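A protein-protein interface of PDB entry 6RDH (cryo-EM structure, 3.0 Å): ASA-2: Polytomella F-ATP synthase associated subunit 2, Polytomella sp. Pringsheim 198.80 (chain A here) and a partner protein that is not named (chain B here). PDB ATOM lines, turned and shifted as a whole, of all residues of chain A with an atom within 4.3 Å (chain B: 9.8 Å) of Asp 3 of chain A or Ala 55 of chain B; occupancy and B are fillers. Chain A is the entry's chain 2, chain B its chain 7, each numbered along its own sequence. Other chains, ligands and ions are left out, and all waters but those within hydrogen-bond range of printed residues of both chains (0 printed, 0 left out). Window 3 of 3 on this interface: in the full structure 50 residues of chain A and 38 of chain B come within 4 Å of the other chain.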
ATOM      1  N   ASN A   2     -16.447  -6.972  36.305  1.00  0.00           N
ATOM      2  CA  ASN A   2     -15.710  -6.024  35.467  1.00  0.00           C
ATOM      3  C   ASN A   2     -14.642  -6.829  34.732  1.00  0.00           C
ATOM      4  O   ASN A   2     -13.649  -7.243  35.339  1.00  0.00           O
ATOM      5  CB  ASN A   2     -15.089  -4.906  36.289  1.00  0.00           C
ATOM      6  CG  ASN A   2     -14.243  -3.970  35.449  1.00  0.00           C
ATOM      7  OD1 ASN A   2     -14.602  -3.631  34.322  1.00  0.00           O
ATOM      8  ND2 ASN A   2     -13.099  -3.569  35.988  1.00  0.00           N
ATOM      9  N   ASP A   3     -14.855  -7.066  33.439  1.00  0.00           N
ATOM     10  CA  ASP A   3     -13.964  -7.927  32.665  1.00  0.00           C
ATOM     11  C   ASP A   3     -13.936  -7.461  31.216  1.00  0.00           C
ATOM     12  O   ASP A   3     -14.964  -7.472  30.535  1.00  0.00           O
ATOM     13  CB  ASP A   3     -14.393  -9.390  32.779  1.00  0.00           C
ATOM     14  CG  ASP A   3     -15.902  -9.560  32.842  1.00  0.00           C
ATOM     15  OD1 ASP A   3     -16.629  -8.557  32.713  1.00  0.00           O
ATOM     16  OD2 ASP A   3     -16.357 -10.699  33.078  1.00  0.00           O
ATOM     17  N   VAL A   4     -12.757  -7.060  30.753  1.00  0.00           N
ATOM     18  CA  VAL A   4     -12.558  -6.556  29.393  1.00  0.00           C
ATOM     19  C   VAL A   4     -12.543  -7.656  28.325  1.00  0.00           C
ATOM     20  O   VAL A   4     -13.330  -7.537  27.373  1.00  0.00           O
ATOM     21  CB  VAL A   4     -11.294  -5.678  29.324  1.00  0.00           C
ATOM     22  CG1 VAL A   4     -10.955  -5.325  27.887  1.00  0.00           C
ATOM     23  CG2 VAL A   4     -11.482  -4.420  30.153  1.00  0.00           C
ATOM     24  N   PRO A   5     -11.722  -8.725  28.391  1.00  0.00           N
ATOM     25  CA  PRO A   5     -11.688  -9.642  27.238  1.00  0.00           C
ATOM     26  C   PRO A   5     -12.927 -10.506  27.110  1.00  0.00           C
ATOM     27  O   PRO A   5     -13.291 -10.889  25.990  1.00  0.00           O
ATOM     28  CB  PRO A   5     -10.439 -10.499  27.495  1.00  0.00           C
ATOM     29  CG  PRO A   5      -9.734  -9.852  28.630  1.00  0.00           C
ATOM     30  CD  PRO A   5     -10.809  -9.239  29.429  1.00  0.00           C
ATOM     31  N   ALA A   6     -13.603 -10.801  28.219  1.00  0.00           N
ATOM     32  CA  ALA A   6     -14.849 -11.550  28.136  1.00  0.00           C
ATOM     33  C   ALA A   6     -15.948 -10.719  27.488  1.00  0.00           C
ATOM     34  O   ALA A   6     -16.742 -11.242  26.699  1.00  0.00           O
ATOM     35  CB  ALA A   6     -15.263 -12.029  29.524  1.00  0.00           C
ATOM     36  N   ILE A   7     -15.981  -9.413  27.754  1.00  0.00           N
ATOM     37  CA  ILE A   7     -16.950  -8.586  27.046  1.00  0.00           C
ATOM     38  C   ILE A   7     -16.517  -8.327  25.610  1.00  0.00           C
ATOM     39  O   ILE A   7     -17.375  -8.080  24.752  1.00  0.00           O
ATOM     40  CB  ILE A   7     -17.233  -7.278  27.805  1.00  0.00           C
ATOM     41  CG1 ILE A   7     -18.638  -6.800  27.495  1.00  0.00           C
ATOM     42  CG2 ILE A   7     -16.285  -6.175  27.438  1.00  0.00           C
ATOM     43  CD1 ILE A   7     -19.099  -5.773  28.438  1.00  0.00           C
ATOM     44  N   SER B  34     -29.412  -5.533  22.809  1.00  0.00           N
ATOM     45  CA  SER B  34     -28.459  -6.635  22.781  1.00  0.00           C
ATOM     46  C   SER B  34     -27.245  -6.342  23.647  1.00  0.00           C
ATOM     47  O   SER B  34     -26.636  -7.265  24.198  1.00  0.00           O
ATOM     48  CB  SER B  34     -28.037  -6.906  21.344  1.00  0.00           C
ATOM     49  OG  SER B  34     -27.325  -5.797  20.837  1.00  0.00           O
ATOM     50  N   ILE B  35     -26.876  -5.075  23.772  1.00  0.00           N
ATOM     51  CA  ILE B  35     -25.822  -4.661  24.688  1.00  0.00           C
ATOM     52  C   ILE B  35     -26.293  -3.382  25.368  1.00  0.00           C
ATOM     53  O   ILE B  35     -26.952  -2.540  24.748  1.00  0.00           O
ATOM     54  CB  ILE B  35     -24.466  -4.502  23.959  1.00  0.00           C
ATOM     55  CG1 ILE B  35     -23.328  -4.185  24.913  1.00  0.00           C
ATOM     56  CG2 ILE B  35     -24.499  -3.444  22.910  1.00  0.00           C
ATOM     57  CD1 ILE B  35     -21.984  -4.264  24.238  1.00  0.00           C
ATOM     58  N   LYS B  36     -26.048  -3.281  26.666  1.00  0.00           N
ATOM     59  CA  LYS B  36     -26.430  -2.096  27.413  1.00  0.00           C
ATOM     60  C   LYS B  36     -25.195  -1.258  27.695  1.00  0.00           C
ATOM     61  O   LYS B  36     -24.147  -1.777  28.085  1.00  0.00           O
ATOM     62  CB  LYS B  36     -27.132  -2.473  28.716  1.00  0.00           C
ATOM     63  CG  LYS B  36     -28.521  -3.061  28.522  1.00  0.00           C
ATOM     64  CD  LYS B  36     -29.397  -2.134  27.692  1.00  0.00           C
ATOM     65  CE  LYS B  36     -30.752  -2.755  27.415  1.00  0.00           C
ATOM     66  NZ  LYS B  36     -31.544  -1.953  26.449  1.00  0.00           N
ATOM     67  N   THR B  49     -20.230   1.972  31.892  1.00  0.00           N
ATOM     68  CA  THR B  49     -20.401   0.574  32.281  1.00  0.00           C
ATOM     69  C   THR B  49     -21.000  -0.113  31.060  1.00  0.00           C
ATOM     70  O   THR B  49     -22.195   0.037  30.791  1.00  0.00           O
ATOM     71  CB  THR B  49     -21.326   0.407  33.483  1.00  0.00           C
ATOM     72  OG1 THR B  49     -22.643   0.831  33.121  1.00  0.00           O
ATOM     73  CG2 THR B  49     -20.865   1.228  34.681  1.00  0.00           C
ATOM     74  N   VAL B  50     -20.186  -0.848  30.316  1.00  0.00           N
ATOM     75  CA  VAL B  50     -20.689  -1.589  29.166  1.00  0.00           C
ATOM     76  C   VAL B  50     -21.211  -2.933  29.657  1.00  0.00           C
ATOM     77  O   VAL B  50     -20.552  -3.613  30.451  1.00  0.00           O
ATOM     78  CB  VAL B  50     -19.591  -1.752  28.105  1.00  0.00           C
ATOM     79  CG1 VAL B  50     -20.092  -2.541  26.934  1.00  0.00           C
ATOM     80  CG2 VAL B  50     -19.103  -0.397  27.641  1.00  0.00           C
ATOM     81  N   ALA B  51     -22.413  -3.305  29.216  1.00  0.00           N
ATOM     82  CA  ALA B  51     -23.110  -4.484  29.722  1.00  0.00           C
ATOM     83  C   ALA B  51     -23.543  -5.360  28.558  1.00  0.00           C
ATOM     84  O   ALA B  51     -24.484  -5.014  27.841  1.00  0.00           O
ATOM     85  CB  ALA B  51     -24.318  -4.081  30.566  1.00  0.00           C
ATOM     86  N   ALA B  52     -22.884  -6.509  28.396  1.00  0.00           N
ATOM     87  CA  ALA B  52     -23.167  -7.445  27.305  1.00  0.00           C
ATOM     88  C   ALA B  52     -23.344  -8.852  27.871  1.00  0.00           C
ATOM     89  O   ALA B  52     -22.372  -9.604  27.991  1.00  0.00           O
ATOM     90  CB  ALA B  52     -22.063  -7.415  26.255  1.00  0.00           C
ATOM     91  N   GLY B  53     -24.588  -9.203  28.199  1.00  0.00           N
ATOM     92  CA  GLY B  53     -24.948 -10.561  28.559  1.00  0.00           C
ATOM     93  C   GLY B  53     -24.373 -11.073  29.862  1.00  0.00           C
ATOM     94  O   GLY B  53     -24.719 -10.583  30.941  1.00  0.00           O
ATOM     95  N   ALA B  54     -23.492 -12.067  29.770  1.00  0.00           N
ATOM     96  CA  ALA B  54     -22.899 -12.655  30.963  1.00  0.00           C
ATOM     97  C   ALA B  54     -21.868 -11.739  31.599  1.00  0.00           C
ATOM     98  O   ALA B  54     -21.901 -11.518  32.814  1.00  0.00           O
ATOM     99  CB  ALA B  54     -22.247 -13.993  30.622  1.00  0.00           C
ATOM    100  N   ALA B  55     -20.962 -11.193  30.802  1.00  0.00           N
ATOM    101  CA  ALA B  55     -19.867 -10.381  31.302  1.00  0.00           C
ATOM    102  C   ALA B  55     -20.139  -8.913  31.027  1.00  0.00           C
ATOM    103  O   ALA B  55     -20.405  -8.531  29.883  1.00  0.00           O
ATOM    104  CB  ALA B  55     -18.554 -10.795  30.652  1.00  0.00           C
ATOM    105  N   LYS B  56     -20.062  -8.095  32.069  1.00  0.00           N
ATOM    106  CA  LYS B  56     -20.170  -6.652  31.935  1.00  0.00           C
ATOM    107  C   LYS B  56     -18.946  -6.003  32.558  1.00  0.00           C
ATOM    108  O   LYS B  56     -18.428  -6.475  33.574  1.00  0.00           O
ATOM    109  CB  LYS B  56     -21.463  -6.118  32.568  1.00  0.00           C
ATOM    110  CG  LYS B  56     -21.646  -6.402  34.046  1.00  0.00           C
ATOM    111  CD  LYS B  56     -23.003  -5.914  34.535  1.00  0.00           C
ATOM    112  CE  LYS B  56     -23.192  -6.233  36.006  1.00  0.00           C
ATOM    113  NZ  LYS B  56     -23.289  -7.698  36.222  1.00  0.00           N
ATOM    114  N   ALA B  57     -18.471  -4.938  31.922  1.00  0.00           N
ATOM    115  CA  ALA B  57     -17.253  -4.259  32.334  1.00  0.00           C
ATOM    116  C   ALA B  57     -17.553  -2.788  32.579  1.00  0.00           C
ATOM    117  O   ALA B  57     -18.533  -2.244  32.067  1.00  0.00           O
ATOM    118  CB  ALA B  57     -16.144  -4.406  31.289  1.00  0.00           C
ATOM    119  N   ALA B  58     -16.702  -2.156  33.382  1.00  0.00           N
ATOM    120  CA  ALA B  58     -16.898  -0.769  33.773  1.00  0.00           C
ATOM    121  C   ALA B  58     -15.552  -0.100  33.971  1.00  0.00           C
ATOM    122  O   ALA B  58     -14.643  -0.695  34.557  1.00  0.00           O
ATOM    123  CB  ALA B  58     -17.721  -0.673  35.056  1.00  0.00           C
ATOM    124  N   THR B  59     -15.430   1.133  33.489  1.00  0.00           N
ATOM    125  CA  THR B  59     -14.221   1.916  33.692  1.00  0.00           C
ATOM    126  C   THR B  59     -14.559   3.397  33.680  1.00  0.00           C
ATOM    127  O   THR B  59     -15.698   3.800  33.429  1.00  0.00           O
ATOM    128  CB  THR B  59     -13.164   1.622  32.629  1.00  0.00           C
ATOM    129  OG1 THR B  59     -12.015   2.442  32.874  1.00  0.00           O
ATOM    130  CG2 THR B  59     -13.711   1.918  31.248  1.00  0.00           C
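Among the printed residues, pairs that only touch across the chains: Asp 3 of chain A with Ala 55 of chain B (3.3 Å), Ile 7 of chain A with Val 50 of chain B (3.3 Å), Asp 3 of chain A with Ala 57 of chain B (3.4 Å), Asn 2 of chain A with Ala 57 of chain B (3.4 Å), Ile 7 of chain A with Ala 55 of chain B (3.4 Å), Ile 7 of chain A with Ala 57 of chain B (3.6 Å), Ala 6 of chain A with Ala 55 of chain B (3.7 Å), Ile 7 of chain A with Ala 52 of chain B (3.7 Å) and Ile 7 of chain A with Lys 56 of chain B (3.8 Å).
The backbone NH (N) of Asn 2 of chain A lies close to the backbone carbonyl oxygen (O) of Lys 56 of chain B, 3.4 Å away.
OD1 of Asn 2 of chain A lies within hydrogen-bond range of N of Ala 58 of chain B (2.7 Å).
O of Lys 56 of chain B lies close to OD1 of Asp 3 of chain A, at 2.9 Å.
N of Val 50 of chain B lies within hydrogen-bond range of O of Ala 57 of chain B, 2.8 Å away.
Asn 2 of chain A touches just these residues of chain B: Lys 56 (3.3 Å), Ala 57 (3.4 Å) and Ala 58 (2.7 Å).
Asp 3 of chain A touches just these residues of chain B: Ala 55, Lys 56 and Ala 57.
Of the printed residues of chain B, Ala 6 of chain A touches Ala 55.
Printed residues of chain B within 4 Å of Ile 7 of chain A: Val 50 (3.3 Å), Ala 52 (3.7 Å), Ala 55 (3.4 Å), Lys 56 (3.8 Å) and Ala 57 (3.6 Å).
Of the printed residues of chain A, Ala 52 of chain B touches Ile 7.
Ala 55 of chain B touches just these residues of chain A: Asp 3, Ala 6 and Ile 7.
Of the printed residues of chain A, Lys 56 of chain B touches Asn 2, Asp 3 and Ile 7.
Of the printed residues of chain A, Ala 57 of chain B touches Asn 2, Asp 3 and Ile 7.
Printed residues of chain A within 4 Å of Ala 58 of chain B: Asn 2 (2.7 Å).
The nearest printed residue of chain A that does not touch Ala 55 of chain B is Pro 5 of chain A (6.7 Å).
Of the 6 printed residues of chain A, 4 touch a printed residue of chain B.
Printed residues of chain A that touch a printed residue of chain B: Asn 2, Asp 3, Ala 6 and Ile 7.
Of the 14 printed residues of chain B, 6 touch a printed residue of chain A.
Hydrophobic or aromatic side chains of chain B within 4 Å of the printed part of chain A: Val 50, Ala 52, Ala 55 and Ala 57.
Among the printed residues, 12 pairs touch across the chains.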
